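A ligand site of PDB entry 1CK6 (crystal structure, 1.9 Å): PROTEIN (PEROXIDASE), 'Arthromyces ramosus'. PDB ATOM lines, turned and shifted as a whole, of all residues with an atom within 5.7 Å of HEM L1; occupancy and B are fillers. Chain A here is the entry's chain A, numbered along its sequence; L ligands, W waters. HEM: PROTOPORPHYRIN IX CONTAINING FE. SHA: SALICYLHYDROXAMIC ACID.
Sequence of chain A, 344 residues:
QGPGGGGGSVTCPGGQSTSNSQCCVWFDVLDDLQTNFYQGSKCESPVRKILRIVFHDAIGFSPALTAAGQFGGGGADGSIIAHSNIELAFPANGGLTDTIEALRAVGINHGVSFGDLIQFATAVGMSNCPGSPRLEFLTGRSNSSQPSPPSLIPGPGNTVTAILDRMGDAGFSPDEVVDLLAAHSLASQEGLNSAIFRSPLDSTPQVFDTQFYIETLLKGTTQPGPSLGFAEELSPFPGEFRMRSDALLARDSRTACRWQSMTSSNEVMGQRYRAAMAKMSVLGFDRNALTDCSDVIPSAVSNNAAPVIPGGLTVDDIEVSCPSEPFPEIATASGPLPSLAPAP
Residues that only touch HEM L1: Gln 189 (3.4 Å), Leu 181 (3.4 Å), Ala 183 (3.5 Å), Phe 55 (3.5 Å), Ala 187 (3.5 Å), Leu 186 (3.5 Å), Leu 51 (3.5 Å), Gly 155 (3.5 Å), Met 243 (3.6 Å), Pro 154 (3.6 Å), Leu 192 (3.6 Å), Pro 156 (3.7 Å), Ser 245 (3.8 Å), Met 277 (3.8 Å), Leu 180 (3.8 Å), Ile 163 (3.9 Å) and Arg 52 (3.9 Å). Hydrophobic or aromatic side chains that line HEM L1: Leu 51, Phe 55, Pro 154, Pro 156, Ile 163, Leu 180, Leu 181, Ala 183, His 184, Ala 187, Leu 192, Met 243 and Met 277. Of the 32 residues printed, 23 come within 4 Å of HEM L1. Along chain A the residues within 4 Å of HEM L1 span positions 48 to 277. The nearest printed residue that does not touch HEM L1 is Tyr 273 (4.2 Å).
NE2 of His 184 is bound to FE of HEM L1 (2.1 Å). The backbone NH (N) of Ser 188 lies within hydrogen-bond range of an oxygen (O2D) of HEM L1, 2.9 Å away. An oxygen (O1A) of HEM L1 is in hydrogen-bond range of the backbone NH (N) of Glu 190, 2.7 Å away. N of Gly 191 is in hydrogen-bond range of O2A of HEM L1 (3.0 Å). An oxygen (O1D) of HEM L1 is in salt-bridge range of the side-chain amino group (NZ) of Lys 49. The guanidinium group (NE) of Arg 52 sits at hydrogen-bond distance from an oxygen (O7) of SHA L2. The guanidinium group of Arg 48 lies within salt-bridge range of an oxygen (O2D) of HEM L1 (3.0 Å). A nitrogen (N8) of SHA L2 sits at hydrogen-bond distance from the backbone carbonyl oxygen of Pro 154 (2.9 Å). The side-chain hydroxyl of Ser 188 sits at hydrogen-bond distance from an oxygen (O2D) of HEM L1, 2.9 Å away.
Water W3 lies within hydrogen-bond range of O1D of HEM L1, OG of Ser 45, OE2 of Glu 190 and NH2 of Arg 48. Water W2 lies within hydrogen-bond range of O1D of HEM L1 (2.8 Å), NZ of Lys 49 (2.9 Å) and NH1 of Arg 52 (2.9 Å). Water W1 lies within hydrogen-bond range of an oxygen (O6) of SHA L2 (2.9 Å) and an oxygen (O2A) of HEM L1 (3.0 Å). Water W5 lies within hydrogen-bond range of O1A of HEM L1 (3.1 Å) and NH1 of Arg 52 (3.3 Å).
The side-chain carboxylate of Glu 190 lies within salt-bridge range of the side-chain amino group of Lys 49, at 2.9 Å. OE1 of Gln 189 is in hydrogen-bond range of N of Leu 192. OE1 of Gln 189 sits at hydrogen-bond distance from N of Gly 191, at 3.4 Å. The backbone NH (N) of Leu 201 sits at hydrogen-bond distance from the backbone carbonyl oxygen (O) of Ala 187 (3.0 Å). O of Pro 156 sits at hydrogen-bond distance from N of Ser 245, at 3.2 Å.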
ATOM      1  N   SER A  45      -2.715 -13.998  16.038  1.00  0.00           N
ATOM      2  CA  SER A  45      -2.405 -15.220  15.305  1.00  0.00           C
ATOM      3  C   SER A  45      -3.371 -16.418  15.523  1.00  0.00           C
ATOM      4  O   SER A  45      -3.731 -16.989  14.492  1.00  0.00           O
ATOM      5  CB  SER A  45      -0.962 -15.605  15.656  1.00  0.00           C
ATOM      6  OG  SER A  45      -0.390 -16.684  14.931  1.00  0.00           O
ATOM      7  N   VAL A  47      -6.618 -16.646  15.875  1.00  0.00           N
ATOM      8  CA  VAL A  47      -7.769 -16.449  14.966  1.00  0.00           C
ATOM      9  C   VAL A  47      -7.333 -16.633  13.497  1.00  0.00           C
ATOM     10  O   VAL A  47      -8.023 -17.297  12.734  1.00  0.00           O
ATOM     11  CB  VAL A  47      -8.391 -15.017  15.111  1.00  0.00           C
ATOM     12  CG1 VAL A  47      -9.579 -14.888  14.161  1.00  0.00           C
ATOM     13  CG2 VAL A  47      -8.889 -14.739  16.520  1.00  0.00           C
ATOM     14  N   ARG A  48      -6.189 -16.101  13.052  1.00  0.00           N
ATOM     15  CA  ARG A  48      -5.763 -16.168  11.652  1.00  0.00           C
ATOM     16  C   ARG A  48      -5.472 -17.603  11.272  1.00  0.00           C
ATOM     17  O   ARG A  48      -5.924 -18.096  10.240  1.00  0.00           O
ATOM     18  CB  ARG A  48      -4.548 -15.247  11.454  1.00  0.00           C
ATOM     19  CG  ARG A  48      -4.864 -13.795  11.843  1.00  0.00           C
ATOM     20  CD  ARG A  48      -3.834 -12.818  11.327  1.00  0.00           C
ATOM     21  NE  ARG A  48      -2.488 -13.194  11.746  1.00  0.00           N
ATOM     22  CZ  ARG A  48      -1.860 -12.638  12.795  1.00  0.00           C
ATOM     23  NH1 ARG A  48      -2.455 -11.701  13.556  1.00  0.00           N
ATOM     24  NH2 ARG A  48      -0.611 -13.065  13.088  1.00  0.00           N
ATOM     25  N   LYS A  49      -4.802 -18.323  12.174  1.00  0.00           N
ATOM     26  CA  LYS A  49      -4.495 -19.732  11.987  1.00  0.00           C
ATOM     27  C   LYS A  49      -5.807 -20.500  11.914  1.00  0.00           C
ATOM     28  O   LYS A  49      -5.912 -21.370  11.025  1.00  0.00           O
ATOM     29  CB  LYS A  49      -3.677 -20.245  13.161  1.00  0.00           C
ATOM     30  CG  LYS A  49      -2.295 -19.621  13.319  1.00  0.00           C
ATOM     31  CD  LYS A  49      -1.428 -20.086  12.169  1.00  0.00           C
ATOM     32  CE  LYS A  49       0.009 -19.710  12.396  1.00  0.00           C
ATOM     33  NZ  LYS A  49       0.825 -20.156  11.281  1.00  0.00           N
ATOM     34  N   LEU A  51      -8.710 -19.522  10.841  1.00  0.00           N
ATOM     35  CA  LEU A  51      -9.347 -19.218   9.577  1.00  0.00           C
ATOM     36  C   LEU A  51      -8.711 -20.000   8.420  1.00  0.00           C
ATOM     37  O   LEU A  51      -9.417 -20.478   7.513  1.00  0.00           O
ATOM     38  CB  LEU A  51      -9.250 -17.720   9.308  1.00  0.00           C
ATOM     39  CG  LEU A  51     -10.298 -16.845  10.004  1.00  0.00           C
ATOM     40  CD1 LEU A  51      -9.949 -15.368   9.796  1.00  0.00           C
ATOM     41  CD2 LEU A  51     -11.683 -17.161   9.421  1.00  0.00           C
ATOM     42  N   ARG A  52      -7.384 -20.159   8.439  1.00  0.00           N
ATOM     43  CA  ARG A  52      -6.672 -20.937   7.417  1.00  0.00           C
ATOM     44  C   ARG A  52      -7.050 -22.412   7.626  1.00  0.00           C
ATOM     45  O   ARG A  52      -7.345 -23.128   6.656  1.00  0.00           O
ATOM     46  CB  ARG A  52      -5.186 -20.643   7.603  1.00  0.00           C
ATOM     47  CG  ARG A  52      -4.333 -21.216   6.534  1.00  0.00           C
ATOM     48  CD  ARG A  52      -2.893 -20.731   6.648  1.00  0.00           C
ATOM     49  NE  ARG A  52      -2.100 -21.732   5.936  1.00  0.00           N
ATOM     50  CZ  ARG A  52      -0.950 -22.217   6.419  1.00  0.00           C
ATOM     51  NH1 ARG A  52      -0.409 -21.804   7.582  1.00  0.00           N
ATOM     52  NH2 ARG A  52      -0.380 -23.237   5.775  1.00  0.00           N
ATOM     53  N   VAL A  54      -9.991 -23.717   8.825  1.00  0.00           N
ATOM     54  CA  VAL A  54     -11.373 -24.059   8.440  1.00  0.00           C
ATOM     55  C   VAL A  54     -11.486 -24.249   6.926  1.00  0.00           C
ATOM     56  O   VAL A  54     -12.146 -25.170   6.413  1.00  0.00           O
ATOM     57  CB  VAL A  54     -12.292 -22.927   9.039  1.00  0.00           C
ATOM     58  CG1 VAL A  54     -12.272 -21.608   8.254  1.00  0.00           C
ATOM     59  CG2 VAL A  54     -13.685 -23.500   9.071  1.00  0.00           C
ATOM     60  N   PHE A  55     -10.719 -23.444   6.194  1.00  0.00           N
ATOM     61  CA  PHE A  55     -10.630 -23.527   4.750  1.00  0.00           C
ATOM     62  C   PHE A  55      -9.929 -24.835   4.429  1.00  0.00           C
ATOM     63  O   PHE A  55     -10.510 -25.626   3.683  1.00  0.00           O
ATOM     64  CB  PHE A  55      -9.811 -22.335   4.156  1.00  0.00           C
ATOM     65  CG  PHE A  55      -9.570 -22.403   2.645  1.00  0.00           C
ATOM     66  CD1 PHE A  55     -10.580 -22.795   1.750  1.00  0.00           C
ATOM     67  CD2 PHE A  55      -8.312 -22.086   2.133  1.00  0.00           C
ATOM     68  CE1 PHE A  55     -10.337 -22.872   0.379  1.00  0.00           C
ATOM     69  CE2 PHE A  55      -8.061 -22.162   0.769  1.00  0.00           C
ATOM     70  CZ  PHE A  55      -9.074 -22.556  -0.108  1.00  0.00           C
ATOM     71  N   PRO A 154      -5.977 -25.114  -2.866  1.00  0.00           N
ATOM     72  CA  PRO A 154      -5.368 -24.095  -3.744  1.00  0.00           C
ATOM     73  C   PRO A 154      -4.077 -23.515  -3.164  1.00  0.00           C
ATOM     74  O   PRO A 154      -3.943 -23.265  -1.945  1.00  0.00           O
ATOM     75  CB  PRO A 154      -6.436 -23.015  -3.913  1.00  0.00           C
ATOM     76  CG  PRO A 154      -7.702 -23.761  -3.665  1.00  0.00           C
ATOM     77  CD  PRO A 154      -7.363 -24.771  -2.560  1.00  0.00           C
ATOM     78  N   GLY A 155      -3.136 -23.272  -4.072  1.00  0.00           N
ATOM     79  CA  GLY A 155      -1.849 -22.744  -3.697  1.00  0.00           C
ATOM     80  C   GLY A 155      -1.621 -21.361  -4.284  1.00  0.00           C
ATOM     81  O   GLY A 155      -2.163 -21.026  -5.349  1.00  0.00           O
ATOM     82  N   PRO A 156      -0.749 -20.550  -3.661  1.00  0.00           N
ATOM     83  CA  PRO A 156      -0.439 -19.179  -4.090  1.00  0.00           C
ATOM     84  C   PRO A 156       0.251 -19.070  -5.444  1.00  0.00           C
ATOM     85  O   PRO A 156       0.215 -18.015  -6.062  1.00  0.00           O
ATOM     86  CB  PRO A 156       0.367 -18.629  -2.949  1.00  0.00           C
ATOM     87  CG  PRO A 156       1.130 -19.831  -2.435  1.00  0.00           C
ATOM     88  CD  PRO A 156       0.077 -20.930  -2.509  1.00  0.00           C
ATOM     89  N   ILE A 163      -7.247 -22.343  -9.719  1.00  0.00           N
ATOM     90  CA  ILE A 163      -8.014 -22.053  -8.511  1.00  0.00           C
ATOM     91  C   ILE A 163      -9.514 -22.105  -8.805  1.00  0.00           C
ATOM     92  O   ILE A 163     -10.257 -22.803  -8.107  1.00  0.00           O
ATOM     93  CB  ILE A 163      -7.602 -20.656  -7.994  1.00  0.00           C
ATOM     94  CG1 ILE A 163      -6.133 -20.750  -7.541  1.00  0.00           C
ATOM     95  CG2 ILE A 163      -8.523 -20.184  -6.875  1.00  0.00           C
ATOM     96  CD1 ILE A 163      -5.466 -19.366  -7.279  1.00  0.00           C
ATOM     97  N   MET A 167     -11.938 -24.741  -6.932  1.00  0.00           N
ATOM     98  CA  MET A 167     -12.998 -24.192  -6.121  1.00  0.00           C
ATOM     99  C   MET A 167     -14.376 -24.507  -6.697  1.00  0.00           C
ATOM    100  O   MET A 167     -15.326 -24.768  -5.961  1.00  0.00           O
ATOM    101  CB  MET A 167     -12.830 -22.686  -6.009  1.00  0.00           C
ATOM    102  CG  MET A 167     -11.619 -22.235  -5.194  1.00  0.00           C
ATOM    103  SD  MET A 167     -11.617 -22.739  -3.445  1.00  0.00           S
ATOM    104  CE  MET A 167     -12.518 -21.430  -2.668  1.00  0.00           C
ATOM    105  N   VAL A 177     -15.604 -17.310  -4.683  1.00  0.00           N
ATOM    106  CA  VAL A 177     -14.177 -17.439  -4.440  1.00  0.00           C
ATOM    107  C   VAL A 177     -13.722 -16.052  -3.993  1.00  0.00           C
ATOM    108  O   VAL A 177     -13.041 -15.931  -2.970  1.00  0.00           O
ATOM    109  CB  VAL A 177     -13.396 -17.835  -5.738  1.00  0.00           C
ATOM    110  CG1 VAL A 177     -11.872 -17.756  -5.484  1.00  0.00           C
ATOM    111  CG2 VAL A 177     -13.829 -19.220  -6.163  1.00  0.00           C
ATOM    112  N   LEU A 180     -14.990 -15.297  -0.426  1.00  0.00           N
ATOM    113  CA  LEU A 180     -14.265 -16.085   0.555  1.00  0.00           C
ATOM    114  C   LEU A 180     -12.914 -15.483   0.959  1.00  0.00           C
ATOM    115  O   LEU A 180     -12.475 -15.546   2.114  1.00  0.00           O
ATOM    116  CB  LEU A 180     -14.121 -17.456  -0.054  1.00  0.00           C
ATOM    117  CG  LEU A 180     -14.656 -18.689   0.658  1.00  0.00           C
ATOM    118  CD1 LEU A 180     -15.761 -18.396   1.637  1.00  0.00           C
ATOM    119  CD2 LEU A 180     -15.099 -19.607  -0.442  1.00  0.00           C
ATOM    120  N   LEU A 181     -12.263 -14.847   0.005  1.00  0.00           N
ATOM    121  CA  LEU A 181     -10.995 -14.209   0.206  1.00  0.00           C
ATOM    122  C   LEU A 181     -11.050 -12.970   1.092  1.00  0.00           C
ATOM    123  O   LEU A 181     -10.015 -12.370   1.388  1.00  0.00           O
ATOM    124  CB  LEU A 181     -10.434 -13.884  -1.154  1.00  0.00           C
ATOM    125  CG  LEU A 181      -9.161 -14.540  -1.671  1.00  0.00           C
ATOM    126  CD1 LEU A 181      -8.562 -15.561  -0.726  1.00  0.00           C
ATOM    127  CD2 LEU A 181      -9.538 -15.108  -2.998  1.00  0.00           C
ATOM    128  N   ALA A 183     -11.359 -13.153   4.044  1.00  0.00           N
ATOM    129  CA  ALA A 183     -10.601 -13.594   5.185  1.00  0.00           C
ATOM    130  C   ALA A 183      -9.130 -13.170   5.105  1.00  0.00           C
ATOM    131  O   ALA A 183      -8.481 -13.084   6.148  1.00  0.00           O
ATOM    132  CB  ALA A 183     -10.672 -15.098   5.287  1.00  0.00           C
ATOM    133  N   HIS A 184      -8.567 -12.800   3.937  1.00  0.00           N
ATOM    134  CA  HIS A 184      -7.210 -12.303   3.892  1.00  0.00           C
ATOM    135  C   HIS A 184      -7.121 -10.852   4.415  1.00  0.00           C
ATOM    136  O   HIS A 184      -6.040 -10.249   4.466  1.00  0.00           O
ATOM    137  CB  HIS A 184      -6.682 -12.395   2.464  1.00  0.00           C
ATOM    138  CG  HIS A 184      -6.168 -13.762   2.038  1.00  0.00           C
ATOM    139  ND1 HIS A 184      -5.475 -13.995   0.870  1.00  0.00           N
ATOM    140  CD2 HIS A 184      -6.286 -14.936   2.779  1.00  0.00           C
ATOM    141  CE1 HIS A 184      -5.177 -15.306   0.895  1.00  0.00           C
ATOM    142  NE2 HIS A 184      -5.618 -15.858   1.972  1.00  0.00           N
ATOM    143  N   LEU A 186      -7.658 -10.381   7.461  1.00  0.00           N
ATOM    144  CA  LEU A 186      -7.217 -10.645   8.833  1.00  0.00           C
ATOM    145  C   LEU A 186      -6.056 -11.618   8.586  1.00  0.00           C
ATOM    146  O   LEU A 186      -6.090 -12.772   9.015  1.00  0.00           O
ATOM    147  CB  LEU A 186      -8.395 -11.309   9.566  1.00  0.00           C
ATOM    148  CG  LEU A 186      -9.386 -10.676  10.583  1.00  0.00           C
ATOM    149  CD1 LEU A 186      -9.358  -9.178  10.567  1.00  0.00           C
ATOM    150  CD2 LEU A 186     -10.761 -11.268  10.287  1.00  0.00           C
ATOM    151  N   ALA A 187      -4.998 -11.227   7.886  1.00  0.00           N
ATOM    152  CA  ALA A 187      -4.001 -12.210   7.507  1.00  0.00           C
ATOM    153  C   ALA A 187      -2.561 -11.784   7.427  1.00  0.00           C
ATOM    154  O   ALA A 187      -2.246 -10.612   7.198  1.00  0.00           O
ATOM    155  CB  ALA A 187      -4.388 -12.756   6.145  1.00  0.00           C
ATOM    156  N   SER A 188      -1.685 -12.736   7.578  1.00  0.00           N
ATOM    157  CA  SER A 188      -0.272 -12.487   7.401  1.00  0.00           C
ATOM    158  C   SER A 188       0.249 -13.767   6.761  1.00  0.00           C
ATOM    159  O   SER A 188      -0.519 -14.719   6.458  1.00  0.00           O
ATOM    160  CB  SER A 188       0.431 -12.262   8.760  1.00  0.00           C
ATOM    161  OG  SER A 188       0.678 -13.442   9.506  1.00  0.00           O
ATOM    162  N   GLN A 189       1.546 -13.824   6.474  1.00  0.00           N
ATOM    163  CA  GLN A 189       2.139 -15.077   6.029  1.00  0.00           C
ATOM    164  C   GLN A 189       3.314 -15.330   6.990  1.00  0.00           C
ATOM    165  O   GLN A 189       3.917 -14.392   7.530  1.00  0.00           O
ATOM    166  CB  GLN A 189       2.648 -14.990   4.574  1.00  0.00           C
ATOM    167  CG  GLN A 189       3.788 -13.990   4.301  1.00  0.00           C
ATOM    168  CD  GLN A 189       5.204 -14.465   4.645  1.00  0.00           C
ATOM    169  OE1 GLN A 189       5.537 -15.640   4.566  1.00  0.00           O
ATOM    170  NE2 GLN A 189       6.093 -13.585   5.031  1.00  0.00           N
ATOM    171  N   GLU A 190       3.731 -16.566   7.159  1.00  0.00           N
ATOM    172  CA  GLU A 190       4.854 -16.886   8.023  1.00  0.00           C
ATOM    173  C   GLU A 190       5.832 -17.777   7.285  1.00  0.00           C
ATOM    174  O   GLU A 190       7.038 -17.727   7.533  1.00  0.00           O
ATOM    175  CB  GLU A 190       4.405 -17.629   9.239  1.00  0.00           C
ATOM    176  CG  GLU A 190       3.561 -16.797  10.204  1.00  0.00           C
ATOM    177  CD  GLU A 190       3.143 -17.517  11.486  1.00  0.00           C
ATOM    178  OE1 GLU A 190       3.347 -18.721  11.624  1.00  0.00           O
ATOM    179  OE2 GLU A 190       2.575 -16.870  12.348  1.00  0.00           O
ATOM    180  N   GLY A 191       5.299 -18.546   6.332  1.00  0.00           N
ATOM    181  CA  GLY A 191       6.105 -19.501   5.602  1.00  0.00           C
ATOM    182  C   GLY A 191       6.419 -19.210   4.152  1.00  0.00           C
ATOM    183  O   GLY A 191       7.110 -20.033   3.540  1.00  0.00           O
ATOM    184  N   LEU A 192       5.935 -18.148   3.528  1.00  0.00           N
ATOM    185  CA  LEU A 192       6.248 -17.861   2.137  1.00  0.00           C
ATOM    186  C   LEU A 192       7.581 -17.102   2.077  1.00  0.00           C
ATOM    187  O   LEU A 192       8.432 -17.308   1.201  1.00  0.00           O
ATOM    188  CB  LEU A 192       5.058 -17.086   1.609  1.00  0.00           C
ATOM    189  CG  LEU A 192       3.941 -17.744   0.791  1.00  0.00           C
ATOM    190  CD1 LEU A 192       3.799 -19.237   1.077  1.00  0.00           C
ATOM    191  CD2 LEU A 192       2.702 -16.913   1.030  1.00  0.00           C
ATOM    192  N   LEU A 201      -1.135  -8.936   5.016  1.00  0.00           N
ATOM    193  CA  LEU A 201      -1.648  -8.929   3.656  1.00  0.00           C
ATOM    194  C   LEU A 201      -2.442  -7.651   3.449  1.00  0.00           C
ATOM    195  O   LEU A 201      -2.795  -7.330   2.296  1.00  0.00           O
ATOM    196  CB  LEU A 201      -2.476 -10.204   3.431  1.00  0.00           C
ATOM    197  CG  LEU A 201      -1.785 -11.417   2.742  1.00  0.00           C
ATOM    198  CD1 LEU A 201      -0.444 -11.749   3.346  1.00  0.00           C
ATOM    199  CD2 LEU A 201      -2.712 -12.609   2.849  1.00  0.00           C
ATOM    200  N   MET A 243       0.825 -11.888  -2.254  1.00  0.00           N
ATOM    201  CA  MET A 243       1.046 -13.203  -2.875  1.00  0.00           C
ATOM    202  C   MET A 243       0.428 -13.203  -4.269  1.00  0.00           C
ATOM    203  O   MET A 243      -0.563 -12.506  -4.550  1.00  0.00           O
ATOM    204  CB  MET A 243       0.441 -14.377  -2.028  1.00  0.00           C
ATOM    205  CG  MET A 243      -1.053 -14.509  -1.866  1.00  0.00           C
ATOM    206  SD  MET A 243      -1.531 -15.899  -0.813  1.00  0.00           S
ATOM    207  CE  MET A 243      -1.168 -15.188   0.712  1.00  0.00           C
ATOM    208  N   SER A 245      -1.442 -15.314  -6.251  1.00  0.00           N
ATOM    209  CA  SER A 245      -2.833 -15.638  -6.501  1.00  0.00           C
ATOM    210  C   SER A 245      -3.760 -14.481  -6.194  1.00  0.00           C
ATOM    211  O   SER A 245      -4.691 -14.250  -6.971  1.00  0.00           O
ATOM    212  CB  SER A 245      -3.215 -16.860  -5.688  1.00  0.00           C
ATOM    213  OG  SER A 245      -2.841 -16.711  -4.318  1.00  0.00           O
ATOM    214  N   LEU A 249      -5.990 -12.718  -8.996  1.00  0.00           N
ATOM    215  CA  LEU A 249      -7.436 -12.744  -8.892  1.00  0.00           C
ATOM    216  C   LEU A 249      -7.967 -11.328  -8.922  1.00  0.00           C
ATOM    217  O   LEU A 249      -9.007 -11.084  -9.521  1.00  0.00           O
ATOM    218  CB  LEU A 249      -7.876 -13.462  -7.602  1.00  0.00           C
ATOM    219  CG  LEU A 249      -7.700 -14.982  -7.632  1.00  0.00           C
ATOM    220  CD1 LEU A 249      -7.751 -15.572  -6.233  1.00  0.00           C
ATOM    221  CD2 LEU A 249      -8.773 -15.565  -8.501  1.00  0.00           C
ATOM    222  N   TYR A 273     -19.366 -12.438   2.562  1.00  0.00           N
ATOM    223  CA  TYR A 273     -18.478 -13.357   3.222  1.00  0.00           C
ATOM    224  C   TYR A 273     -19.284 -14.267   4.132  1.00  0.00           C
ATOM    225  O   TYR A 273     -19.048 -15.476   4.110  1.00  0.00           O
ATOM    226  CB  TYR A 273     -17.437 -12.573   4.005  1.00  0.00           C
ATOM    227  CG  TYR A 273     -16.508 -13.453   4.834  1.00  0.00           C
ATOM    228  CD1 TYR A 273     -15.440 -14.151   4.228  1.00  0.00           C
ATOM    229  CD2 TYR A 273     -16.722 -13.530   6.219  1.00  0.00           C
ATOM    230  CE1 TYR A 273     -14.574 -14.911   5.022  1.00  0.00           C
ATOM    231  CE2 TYR A 273     -15.864 -14.290   7.006  1.00  0.00           C
ATOM    232  CZ  TYR A 273     -14.804 -14.968   6.407  1.00  0.00           C
ATOM    233  OH  TYR A 273     -13.937 -15.670   7.195  1.00  0.00           O
ATOM    234  N   MET A 277     -19.217 -18.367   3.664  1.00  0.00           N
ATOM    235  CA  MET A 277     -18.737 -19.169   4.793  1.00  0.00           C
ATOM    236  C   MET A 277     -19.806 -20.142   5.262  1.00  0.00           C
ATOM    237  O   MET A 277     -19.472 -21.269   5.645  1.00  0.00           O
ATOM    238  CB  MET A 277     -18.359 -18.326   5.993  1.00  0.00           C
ATOM    239  CG  MET A 277     -17.031 -17.595   5.812  1.00  0.00           C
ATOM    240  SD  MET A 277     -15.611 -18.708   5.617  1.00  0.00           S
ATOM    241  CE  MET A 277     -15.311 -19.005   7.345  1.00  0.00           C
ATOM    242  N   MET A 280     -19.529 -22.988   2.859  1.00  0.00           N
ATOM    243  CA  MET A 280     -18.333 -23.758   3.112  1.00  0.00           C
ATOM    244  C   MET A 280     -18.452 -24.622   4.364  1.00  0.00           C
ATOM    245  O   MET A 280     -17.925 -25.728   4.368  1.00  0.00           O
ATOM    246  CB  MET A 280     -17.137 -22.834   3.258  1.00  0.00           C
ATOM    247  CG  MET A 280     -15.846 -23.648   3.334  1.00  0.00           C
ATOM    248  SD  MET A 280     -14.314 -22.752   3.089  1.00  0.00           S
ATOM    249  CE  MET A 280     -14.373 -21.990   4.664  1.00  0.00           C
HETATM  250  CHA HEM L   1      -2.855 -17.121   4.716  1.00  0.00           C
HETATM  251  CHB HEM L   1      -3.206 -19.008   0.284  1.00  0.00           C
HETATM  252  CHC HEM L   1      -7.988 -18.702   0.519  1.00  0.00           C
HETATM  253  CHD HEM L   1      -7.631 -17.547   5.172  1.00  0.00           C
HETATM  254  C1A HEM L   1      -2.526 -17.660   3.474  1.00  0.00           C
HETATM  255  C2A HEM L   1      -1.187 -18.018   3.060  1.00  0.00           C
HETATM  256  C3A HEM L   1      -1.297 -18.563   1.818  1.00  0.00           C
HETATM  257  C4A HEM L   1      -2.694 -18.560   1.486  1.00  0.00           C
HETATM  258  CMA HEM L   1      -0.183 -19.047   0.905  1.00  0.00           C
HETATM  259  CAA HEM L   1       0.072 -17.796   3.878  1.00  0.00           C
HETATM  260  CBA HEM L   1       0.294 -18.838   4.962  1.00  0.00           C
HETATM  261  CGA HEM L   1       1.635 -18.664   5.630  1.00  0.00           C
HETATM  262  O1A HEM L   1       1.691 -18.353   6.806  1.00  0.00           O
HETATM  263  O2A HEM L   1       2.655 -18.806   4.962  1.00  0.00           O
HETATM  264  C1B HEM L   1      -4.535 -18.962  -0.092  1.00  0.00           C
HETATM  265  C2B HEM L   1      -5.031 -19.358  -1.387  1.00  0.00           C
HETATM  266  C3B HEM L   1      -6.377 -19.264  -1.339  1.00  0.00           C
HETATM  267  C4B HEM L   1      -6.704 -18.753  -0.011  1.00  0.00           C
HETATM  268  CMB HEM L   1      -4.231 -19.779  -2.602  1.00  0.00           C
HETATM  269  CAB HEM L   1      -7.249 -19.712  -2.351  1.00  0.00           C
HETATM  270  CBB HEM L   1      -7.980 -18.885  -3.288  1.00  0.00           C
HETATM  271  C1C HEM L   1      -8.317 -18.449   1.846  1.00  0.00           C
HETATM  272  C2C HEM L   1      -9.647 -18.623   2.400  1.00  0.00           C
HETATM  273  C3C HEM L   1      -9.541 -18.372   3.732  1.00  0.00           C
HETATM  274  C4C HEM L   1      -8.145 -18.018   3.973  1.00  0.00           C
HETATM  275  CMC HEM L   1     -10.884 -19.022   1.593  1.00  0.00           C
HETATM  276  CAC HEM L   1     -10.502 -18.511   4.764  1.00  0.00           C
HETATM  277  CBC HEM L   1     -11.925 -18.342   4.684  1.00  0.00           C
HETATM  278  C1D HEM L   1      -6.304 -17.191   5.427  1.00  0.00           C
HETATM  279  C2D HEM L   1      -5.830 -16.533   6.619  1.00  0.00           C
HETATM  280  C3D HEM L   1      -4.507 -16.438   6.490  1.00  0.00           C
HETATM  281  C4D HEM L   1      -4.150 -16.977   5.206  1.00  0.00           C
HETATM  282  CMD HEM L   1      -6.693 -15.951   7.739  1.00  0.00           C
HETATM  283  CAD HEM L   1      -3.554 -15.848   7.494  1.00  0.00           C
HETATM  284  CBD HEM L   1      -2.857 -16.865   8.396  1.00  0.00           C
HETATM  285  CGD HEM L   1      -1.878 -16.217   9.368  1.00  0.00           C
HETATM  286  O1D HEM L   1      -1.163 -16.923  10.067  1.00  0.00           O
HETATM  287  O2D HEM L   1      -1.816 -14.992   9.444  1.00  0.00           O
HETATM  288  NA  HEM L   1      -3.453 -18.019   2.508  1.00  0.00           N
HETATM  289  NB  HEM L   1      -5.554 -18.552   0.747  1.00  0.00           N
HETATM  290  NC  HEM L   1      -7.397 -18.106   2.821  1.00  0.00           N
HETATM  291  ND  HEM L   1      -5.275 -17.380   4.527  1.00  0.00           N
HETATM  292 FE   HEM L   1      -5.422 -17.873   2.621  1.00  0.00          FE
HETATM  293  C1  SHA L   2      -0.912 -22.824   0.864  1.00  0.00           C
HETATM  294  C2  SHA L   2      -0.960 -23.584  -0.335  1.00  0.00           C
HETATM  295  C3  SHA L   2       0.192 -24.053  -0.948  1.00  0.00           C
HETATM  296  C4  SHA L   2       1.460 -23.769  -0.387  1.00  0.00           C
HETATM  297  C5  SHA L   2       1.555 -23.028   0.795  1.00  0.00           C
HETATM  298  C6  SHA L   2       0.382 -22.551   1.428  1.00  0.00           C
HETATM  299  O6  SHA L   2       0.503 -21.863   2.602  1.00  0.00           O
HETATM  300  C7  SHA L   2      -2.224 -22.364   1.438  1.00  0.00           C
HETATM  301  O7  SHA L   2      -2.304 -21.911   2.624  1.00  0.00           O
HETATM  302  N8  SHA L   2      -3.343 -22.413   0.734  1.00  0.00           N
HETATM  303  O9  SHA L   2      -4.529 -21.978   1.327  1.00  0.00           O
HETATM  304  O   HOH W   1       2.908 -21.663   4.175  1.00  0.00           O
HETATM  305  O   HOH W   2      -0.137 -19.146   8.757  1.00  0.00           O
HETATM  306  O   HOH W   3      -0.063 -15.995  12.282  1.00  0.00           O
HETATM  307  O   HOH W   4      -4.997 -20.501   3.555  1.00  0.00           O
HETATM  308  O   HOH W   5       2.723 -20.925   8.276  1.00  0.00           O
